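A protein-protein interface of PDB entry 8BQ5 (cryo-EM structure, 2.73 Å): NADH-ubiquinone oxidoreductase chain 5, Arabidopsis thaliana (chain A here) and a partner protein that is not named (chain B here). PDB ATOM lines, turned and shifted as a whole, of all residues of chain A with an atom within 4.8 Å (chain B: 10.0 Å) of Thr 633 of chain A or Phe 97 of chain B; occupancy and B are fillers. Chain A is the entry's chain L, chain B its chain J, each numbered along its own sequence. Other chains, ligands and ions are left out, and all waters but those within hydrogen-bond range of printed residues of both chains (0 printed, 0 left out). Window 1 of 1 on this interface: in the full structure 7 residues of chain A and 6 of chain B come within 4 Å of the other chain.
The backbone carbonyl oxygen of Leu 629 of chain A sits at hydrogen-bond distance from the side-chain hydroxyl of Thr 633 of chain A, at 2.8 Å. O of Thr 633 of chain A lies within hydrogen-bond range of OG1 of Thr 637 of chain A (2.5 Å). The side-chain hydroxyl of Thr 637 of chain A lies within hydrogen-bond range of the backbone carbonyl oxygen of Leu 634 of chain A (3.0 Å).
Leu 629 of chain A touches Phe 97 of chain B. CD2 of Leu 632 of chain A touches CZ of Phe 97 of chain B, 3.7 Å away. OG1 of Thr 633 of chain A touches CD1 of Ile 93 of chain B, 3.5 Å away. Phe 97 of chain B touches Thr 633 of chain A (CE1 to OG1, 3.5 Å). Glu 100 of chain B touches Val 636 of chain A. CD1 of Ile 96 of chain B touches CG2 of Thr 637 of chain A (3.7 Å).
Of chain B, only Phe 97 (3.7 Å) comes within 4 Å of Leu 632 of chain A. Of chain B, only Ile 93 (3.5 Å) and Phe 97 (3.5 Å) come within 4 Å of Thr 633 of chain A. Of the printed residues of chain B, Thr 637 of chain A touches Ile 96 (3.7 Å). Of the printed residues of chain A, Ile 93 of chain B touches Thr 633. Leu 95 of chain B touches none of the printed residues of chain A. Phe 97 of chain B touches just these residues of chain A: Leu 629, Leu 632 and Thr 633. Printed residues of chain A within 4 Å of Glu 100 of chain B: Val 636 (3.8 Å). Phe 102 of chain B touches none of the printed residues of chain A.
Of the 9 printed residues of chain A, 5 touch a printed residue of chain B. Hydrophobic or aromatic side chains of chain B that line the printed part of chain A: Ile 93, Ile 96 and Phe 97. Among the printed residues, no Asp or Glu carboxylate lies within 4 Å of a Lys or Arg side-chain nitrogen of the other chain.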
ATOM      1  N   LEU A 629      11.759 -12.872  35.304  1.00  0.00           N
ATOM      2  CA  LEU A 629      12.447 -12.298  34.151  1.00  0.00           C
ATOM      3  C   LEU A 629      11.501 -12.132  32.967  1.00  0.00           C
ATOM      4  O   LEU A 629      11.524 -11.102  32.282  1.00  0.00           O
ATOM      5  CB  LEU A 629      13.635 -13.180  33.775  1.00  0.00           C
ATOM      6  CG  LEU A 629      14.484 -12.777  32.574  1.00  0.00           C
ATOM      7  CD1 LEU A 629      14.837 -11.298  32.620  1.00  0.00           C
ATOM      8  CD2 LEU A 629      15.733 -13.633  32.535  1.00  0.00           C
ATOM      9  N   LEU A 630      10.661 -13.137  32.712  1.00  0.00           N
ATOM     10  CA  LEU A 630       9.704 -13.050  31.616  1.00  0.00           C
ATOM     11  C   LEU A 630       8.664 -11.969  31.875  1.00  0.00           C
ATOM     12  O   LEU A 630       8.212 -11.299  30.943  1.00  0.00           O
ATOM     13  CB  LEU A 630       9.027 -14.402  31.404  1.00  0.00           C
ATOM     14  CG  LEU A 630       9.779 -15.432  30.563  1.00  0.00           C
ATOM     15  CD1 LEU A 630       8.980 -16.719  30.487  1.00  0.00           C
ATOM     16  CD2 LEU A 630      10.055 -14.889  29.170  1.00  0.00           C
ATOM     17  N   GLY A 631       8.266 -11.788  33.136  1.00  0.00           N
ATOM     18  CA  GLY A 631       7.332 -10.722  33.457  1.00  0.00           C
ATOM     19  C   GLY A 631       7.927  -9.347  33.231  1.00  0.00           C
ATOM     20  O   GLY A 631       7.271  -8.457  32.684  1.00  0.00           O
ATOM     21  N   LEU A 632       9.184  -9.158  33.641  1.00  0.00           N
ATOM     22  CA  LEU A 632       9.870  -7.898  33.363  1.00  0.00           C
ATOM     23  C   LEU A 632       9.992  -7.654  31.861  1.00  0.00           C
ATOM     24  O   LEU A 632       9.765  -6.533  31.382  1.00  0.00           O
ATOM     25  CB  LEU A 632      11.248  -7.906  34.024  1.00  0.00           C
ATOM     26  CG  LEU A 632      12.160  -6.693  33.824  1.00  0.00           C
ATOM     27  CD1 LEU A 632      11.594  -5.454  34.495  1.00  0.00           C
ATOM     28  CD2 LEU A 632      13.556  -7.000  34.342  1.00  0.00           C
ATOM     29  N   THR A 633      10.348  -8.694  31.102  1.00  0.00           N
ATOM     30  CA  THR A 633      10.467  -8.553  29.653  1.00  0.00           C
ATOM     31  C   THR A 633       9.127  -8.210  29.016  1.00  0.00           C
ATOM     32  O   THR A 633       9.057  -7.365  28.118  1.00  0.00           O
ATOM     33  CB  THR A 633      11.030  -9.834  29.041  1.00  0.00           C
ATOM     34  OG1 THR A 633      12.237 -10.199  29.719  1.00  0.00           O
ATOM     35  CG2 THR A 633      11.330  -9.629  27.565  1.00  0.00           C
ATOM     36  N   LEU A 634       8.051  -8.867  29.459  1.00  0.00           N
ATOM     37  CA  LEU A 634       6.726  -8.565  28.932  1.00  0.00           C
ATOM     38  C   LEU A 634       6.326  -7.134  29.255  1.00  0.00           C
ATOM     39  O   LEU A 634       5.764  -6.433  28.404  1.00  0.00           O
ATOM     40  CB  LEU A 634       5.699  -9.551  29.487  1.00  0.00           C
ATOM     41  CG  LEU A 634       4.242  -9.308  29.084  1.00  0.00           C
ATOM     42  CD1 LEU A 634       4.000  -9.779  27.661  1.00  0.00           C
ATOM     43  CD2 LEU A 634       3.288  -9.998  30.046  1.00  0.00           C
ATOM     44  N   PHE A 635       6.613  -6.680  30.478  1.00  0.00           N
ATOM     45  CA  PHE A 635       6.322  -5.297  30.842  1.00  0.00           C
ATOM     46  C   PHE A 635       7.027  -4.332  29.905  1.00  0.00           C
ATOM     47  O   PHE A 635       6.397  -3.436  29.326  1.00  0.00           O
ATOM     48  CB  PHE A 635       6.747  -5.034  32.286  1.00  0.00           C
ATOM     49  CG  PHE A 635       5.685  -5.339  33.294  1.00  0.00           C
ATOM     50  CD1 PHE A 635       4.599  -6.124  32.959  1.00  0.00           C
ATOM     51  CD2 PHE A 635       5.770  -4.830  34.577  1.00  0.00           C
ATOM     52  CE1 PHE A 635       3.620  -6.405  33.887  1.00  0.00           C
ATOM     53  CE2 PHE A 635       4.792  -5.105  35.509  1.00  0.00           C
ATOM     54  CZ  PHE A 635       3.717  -5.894  35.163  1.00  0.00           C
ATOM     55  N   VAL A 636       8.339  -4.512  29.731  1.00  0.00           N
ATOM     56  CA  VAL A 636       9.106  -3.615  28.870  1.00  0.00           C
ATOM     57  C   VAL A 636       8.550  -3.638  27.451  1.00  0.00           C
ATOM     58  O   VAL A 636       8.269  -2.589  26.856  1.00  0.00           O
ATOM     59  CB  VAL A 636      10.598  -3.993  28.892  1.00  0.00           C
ATOM     60  CG1 VAL A 636      11.304  -3.424  27.674  1.00  0.00           C
ATOM     61  CG2 VAL A 636      11.256  -3.509  30.174  1.00  0.00           C
ATOM     62  N   THR A 637       8.351  -4.840  26.902  1.00  0.00           N
ATOM     63  CA  THR A 637       7.954  -4.970  25.504  1.00  0.00           C
ATOM     64  C   THR A 637       6.578  -4.367  25.255  1.00  0.00           C
ATOM     65  O   THR A 637       6.362  -3.689  24.246  1.00  0.00           O
ATOM     66  CB  THR A 637       7.969  -6.440  25.081  1.00  0.00           C
ATOM     67  OG1 THR A 637       7.536  -7.261  26.171  1.00  0.00           O
ATOM     68  CG2 THR A 637       9.363  -6.862  24.654  1.00  0.00           C
ATOM     69  N   VAL B  89      16.410 -18.574  23.614  1.00  0.00           N
ATOM     70  CA  VAL B  89      15.745 -17.770  24.640  1.00  0.00           C
ATOM     71  C   VAL B  89      16.670 -16.664  25.131  1.00  0.00           C
ATOM     72  O   VAL B  89      16.245 -15.514  25.318  1.00  0.00           O
ATOM     73  CB  VAL B  89      15.236 -18.659  25.794  1.00  0.00           C
ATOM     74  CG1 VAL B  89      16.385 -19.250  26.609  1.00  0.00           C
ATOM     75  CG2 VAL B  89      14.288 -17.873  26.686  1.00  0.00           C
ATOM     76  N   SER B  90      17.949 -16.987  25.343  1.00  0.00           N
ATOM     77  CA  SER B  90      18.909 -15.960  25.717  1.00  0.00           C
ATOM     78  C   SER B  90      19.099 -14.961  24.591  1.00  0.00           C
ATOM     79  O   SER B  90      19.239 -13.767  24.852  1.00  0.00           O
ATOM     80  CB  SER B  90      20.247 -16.585  26.109  1.00  0.00           C
ATOM     81  OG  SER B  90      20.861 -17.225  25.005  1.00  0.00           O
ATOM     82  N   GLY B  91      19.086 -15.422  23.340  1.00  0.00           N
ATOM     83  CA  GLY B  91      19.162 -14.490  22.229  1.00  0.00           C
ATOM     84  C   GLY B  91      18.022 -13.491  22.238  1.00  0.00           C
ATOM     85  O   GLY B  91      18.241 -12.283  22.134  1.00  0.00           O
ATOM     86  N   ILE B  92      16.791 -13.980  22.405  1.00  0.00           N
ATOM     87  CA  ILE B  92      15.624 -13.101  22.397  1.00  0.00           C
ATOM     88  C   ILE B  92      15.682 -12.122  23.564  1.00  0.00           C
ATOM     89  O   ILE B  92      15.555 -10.903  23.380  1.00  0.00           O
ATOM     90  CB  ILE B  92      14.328 -13.933  22.427  1.00  0.00           C
ATOM     91  CG1 ILE B  92      13.884 -14.297  21.011  1.00  0.00           C
ATOM     92  CG2 ILE B  92      13.212 -13.181  23.138  1.00  0.00           C
ATOM     93  CD1 ILE B  92      13.048 -15.556  20.949  1.00  0.00           C
ATOM     94  N   ILE B  93      15.891 -12.636  24.779  1.00  0.00           N
ATOM     95  CA  ILE B  93      15.868 -11.770  25.954  1.00  0.00           C
ATOM     96  C   ILE B  93      17.010 -10.763  25.888  1.00  0.00           C
ATOM     97  O   ILE B  93      16.822  -9.570  26.164  1.00  0.00           O
ATOM     98  CB  ILE B  93      15.920 -12.611  27.244  1.00  0.00           C
ATOM     99  CG1 ILE B  93      14.695 -13.525  27.348  1.00  0.00           C
ATOM    100  CG2 ILE B  93      15.993 -11.709  28.462  1.00  0.00           C
ATOM    101  CD1 ILE B  93      13.402 -12.799  27.636  1.00  0.00           C
ATOM    102  N   GLY B  94      18.203 -11.219  25.502  1.00  0.00           N
ATOM    103  CA  GLY B  94      19.346 -10.330  25.430  1.00  0.00           C
ATOM    104  C   GLY B  94      19.204  -9.278  24.350  1.00  0.00           C
ATOM    105  O   GLY B  94      19.623  -8.140  24.531  1.00  0.00           O
ATOM    106  N   LEU B  95      18.604  -9.639  23.213  1.00  0.00           N
ATOM    107  CA  LEU B  95      18.419  -8.662  22.143  1.00  0.00           C
ATOM    108  C   LEU B  95      17.388  -7.610  22.533  1.00  0.00           C
ATOM    109  O   LEU B  95      17.580  -6.412  22.287  1.00  0.00           O
ATOM    110  CB  LEU B  95      18.010  -9.370  20.853  1.00  0.00           C
ATOM    111  CG  LEU B  95      18.434  -8.691  19.547  1.00  0.00           C
ATOM    112  CD1 LEU B  95      19.880  -9.031  19.196  1.00  0.00           C
ATOM    113  CD2 LEU B  95      17.492  -9.072  18.417  1.00  0.00           C
ATOM    114  N   ILE B  96      16.285  -8.040  23.153  1.00  0.00           N
ATOM    115  CA  ILE B  96      15.288  -7.086  23.633  1.00  0.00           C
ATOM    116  C   ILE B  96      15.910  -6.140  24.650  1.00  0.00           C
ATOM    117  O   ILE B  96      15.800  -4.910  24.536  1.00  0.00           O
ATOM    118  CB  ILE B  96      14.075  -7.828  24.224  1.00  0.00           C
ATOM    119  CG1 ILE B  96      13.379  -8.655  23.140  1.00  0.00           C
ATOM    120  CG2 ILE B  96      13.122  -6.855  24.902  1.00  0.00           C
ATOM    121  CD1 ILE B  96      12.045  -9.228  23.562  1.00  0.00           C
ATOM    122  N   PHE B  97      16.590  -6.704  25.652  1.00  0.00           N
ATOM    123  CA  PHE B  97      17.217  -5.882  26.678  1.00  0.00           C
ATOM    124  C   PHE B  97      18.275  -4.970  26.076  1.00  0.00           C
ATOM    125  O   PHE B  97      18.380  -3.801  26.451  1.00  0.00           O
ATOM    126  CB  PHE B  97      17.826  -6.772  27.758  1.00  0.00           C
ATOM    127  CG  PHE B  97      16.922  -7.010  28.927  1.00  0.00           C
ATOM    128  CD1 PHE B  97      16.075  -8.104  28.950  1.00  0.00           C
ATOM    129  CD2 PHE B  97      16.910  -6.138  30.000  1.00  0.00           C
ATOM    130  CE1 PHE B  97      15.239  -8.329  30.024  1.00  0.00           C
ATOM    131  CE2 PHE B  97      16.076  -6.355  31.078  1.00  0.00           C
ATOM    132  CZ  PHE B  97      15.238  -7.451  31.089  1.00  0.00           C
ATOM    133  N   TRP B  98      19.053  -5.483  25.124  1.00  0.00           N
ATOM    134  CA  TRP B  98      20.097  -4.693  24.490  1.00  0.00           C
ATOM    135  C   TRP B  98      19.520  -3.480  23.781  1.00  0.00           C
ATOM    136  O   TRP B  98      19.910  -2.341  24.061  1.00  0.00           O
ATOM    137  CB  TRP B  98      20.879  -5.572  23.515  1.00  0.00           C
ATOM    138  CG  TRP B  98      21.812  -4.815  22.630  1.00  0.00           C
ATOM    139  CD1 TRP B  98      23.051  -4.345  22.949  1.00  0.00           C
ATOM    140  CD2 TRP B  98      21.574  -4.435  21.271  1.00  0.00           C
ATOM    141  NE1 TRP B  98      23.602  -3.697  21.868  1.00  0.00           N
ATOM    142  CE2 TRP B  98      22.713  -3.738  20.826  1.00  0.00           C
ATOM    143  CE3 TRP B  98      20.506  -4.618  20.387  1.00  0.00           C
ATOM    144  CZ2 TRP B  98      22.813  -3.224  19.537  1.00  0.00           C
ATOM    145  CZ3 TRP B  98      20.609  -4.107  19.109  1.00  0.00           C
ATOM    146  CH2 TRP B  98      21.755  -3.419  18.695  1.00  0.00           C
ATOM    147  N   TRP B  99      18.559  -3.701  22.883  1.00  0.00           N
ATOM    148  CA  TRP B  99      18.022  -2.585  22.115  1.00  0.00           C
ATOM    149  C   TRP B  99      17.289  -1.596  23.012  1.00  0.00           C
ATOM    150  O   TRP B  99      17.429  -0.381  22.829  1.00  0.00           O
ATOM    151  CB  TRP B  99      17.137  -3.117  20.978  1.00  0.00           C
ATOM    152  CG  TRP B  99      15.985  -2.243  20.517  1.00  0.00           C
ATOM    153  CD1 TRP B  99      15.954  -0.878  20.436  1.00  0.00           C
ATOM    154  CD2 TRP B  99      14.741  -2.698  19.969  1.00  0.00           C
ATOM    155  NE1 TRP B  99      14.748  -0.458  19.938  1.00  0.00           N
ATOM    156  CE2 TRP B  99      13.988  -1.555  19.633  1.00  0.00           C
ATOM    157  CE3 TRP B  99      14.182  -3.960  19.751  1.00  0.00           C
ATOM    158  CZ2 TRP B  99      12.707  -1.638  19.092  1.00  0.00           C
ATOM    159  CZ3 TRP B  99      12.912  -4.039  19.213  1.00  0.00           C
ATOM    160  CH2 TRP B  99      12.188  -2.886  18.892  1.00  0.00           C
ATOM    161  N   GLU B 100      16.538  -2.073  24.001  1.00  0.00           N
ATOM    162  CA  GLU B 100      15.809  -1.119  24.823  1.00  0.00           C
ATOM    163  C   GLU B 100      16.706  -0.403  25.829  1.00  0.00           C
ATOM    164  O   GLU B 100      16.410   0.732  26.218  1.00  0.00           O
ATOM    165  CB  GLU B 100      14.660  -1.826  25.550  1.00  0.00           C
ATOM    166  CG  GLU B 100      13.758  -0.896  26.340  1.00  0.00           C
ATOM    167  CD  GLU B 100      12.823  -0.102  25.443  1.00  0.00           C
ATOM    168  OE1 GLU B 100      12.177  -0.711  24.566  1.00  0.00           O
ATOM    169  OE2 GLU B 100      12.734   1.133  25.615  1.00  0.00           O
ATOM    170  N   MET B 101      17.829  -1.011  26.226  1.00  0.00           N
ATOM    171  CA  MET B 101      18.493  -0.615  27.453  1.00  0.00           C
ATOM    172  C   MET B 101      19.920  -0.109  27.271  1.00  0.00           C
ATOM    173  O   MET B 101      20.381   0.678  28.102  1.00  0.00           O
ATOM    174  CB  MET B 101      18.483  -1.804  28.425  1.00  0.00           C
ATOM    175  CG  MET B 101      18.498  -1.420  29.871  1.00  0.00           C
ATOM    176  SD  MET B 101      16.947  -0.752  30.490  1.00  0.00           S
ATOM    177  CE  MET B 101      15.769  -1.762  29.606  1.00  0.00           C
ATOM    178  N   PHE B 102      20.633  -0.531  26.221  1.00  0.00           N
ATOM    179  CA  PHE B 102      21.921   0.080  25.910  1.00  0.00           C
ATOM    180  C   PHE B 102      21.787   1.446  25.252  1.00  0.00           C
ATOM    181  O   PHE B 102      22.776   2.183  25.183  1.00  0.00           O
ATOM    182  CB  PHE B 102      22.758  -0.832  25.006  1.00  0.00           C
ATOM    183  CG  PHE B 102      23.277  -2.066  25.686  1.00  0.00           C
ATOM    184  CD1 PHE B 102      24.633  -2.221  25.905  1.00  0.00           C
ATOM    185  CD2 PHE B 102      22.422  -3.060  26.115  1.00  0.00           C
ATOM    186  CE1 PHE B 102      25.125  -3.349  26.527  1.00  0.00           C
ATOM    187  CE2 PHE B 102      22.907  -4.193  26.736  1.00  0.00           C
ATOM    188  CZ  PHE B 102      24.260  -4.335  26.944  1.00  0.00           C
ATOM    189  N   PHE B 103      20.599   1.798  24.763  1.00  0.00           N
ATOM    190  CA  PHE B 103      20.365   3.101  24.156  1.00  0.00           C
ATOM    191  C   PHE B 103      19.338   3.917  24.928  1.00  0.00           C
ATOM    192  O   PHE B 103      18.627   4.734  24.329  1.00  0.00           O
ATOM    193  CB  PHE B 103      19.932   2.932  22.696  1.00  0.00           C
ATOM    194  CG  PHE B 103      20.723   1.891  21.956  1.00  0.00           C
ATOM    195  CD1 PHE B 103      22.024   2.147  21.555  1.00  0.00           C
ATOM    196  CD2 PHE B 103      20.175   0.651  21.681  1.00  0.00           C
ATOM    197  CE1 PHE B 103      22.759   1.188  20.884  1.00  0.00           C
ATOM    198  CE2 PHE B 103      20.905  -0.310  21.012  1.00  0.00           C
ATOM    199  CZ  PHE B 103      22.199  -0.040  20.614  1.00  0.00           C
ATOM    200  N   ILE B 104      19.249   3.724  26.245  1.00  0.00           N
ATOM    201  CA  ILE B 104      18.250   4.433  27.035  1.00  0.00           C
ATOM    202  C   ILE B 104      18.674   5.877  27.268  1.00  0.00           C
ATOM    203  O   ILE B 104      17.826   6.752  27.479  1.00  0.00           O
ATOM    204  CB  ILE B 104      18.003   3.677  28.352  1.00  0.00           C
ATOM    205  CG1 ILE B 104      16.796   4.238  29.093  1.00  0.00           C
ATOM    206  CG2 ILE B 104      19.189   3.829  29.249  1.00  0.00           C
ATOM    207  CD1 ILE B 104      16.676   3.734  30.476  1.00  0.00           C
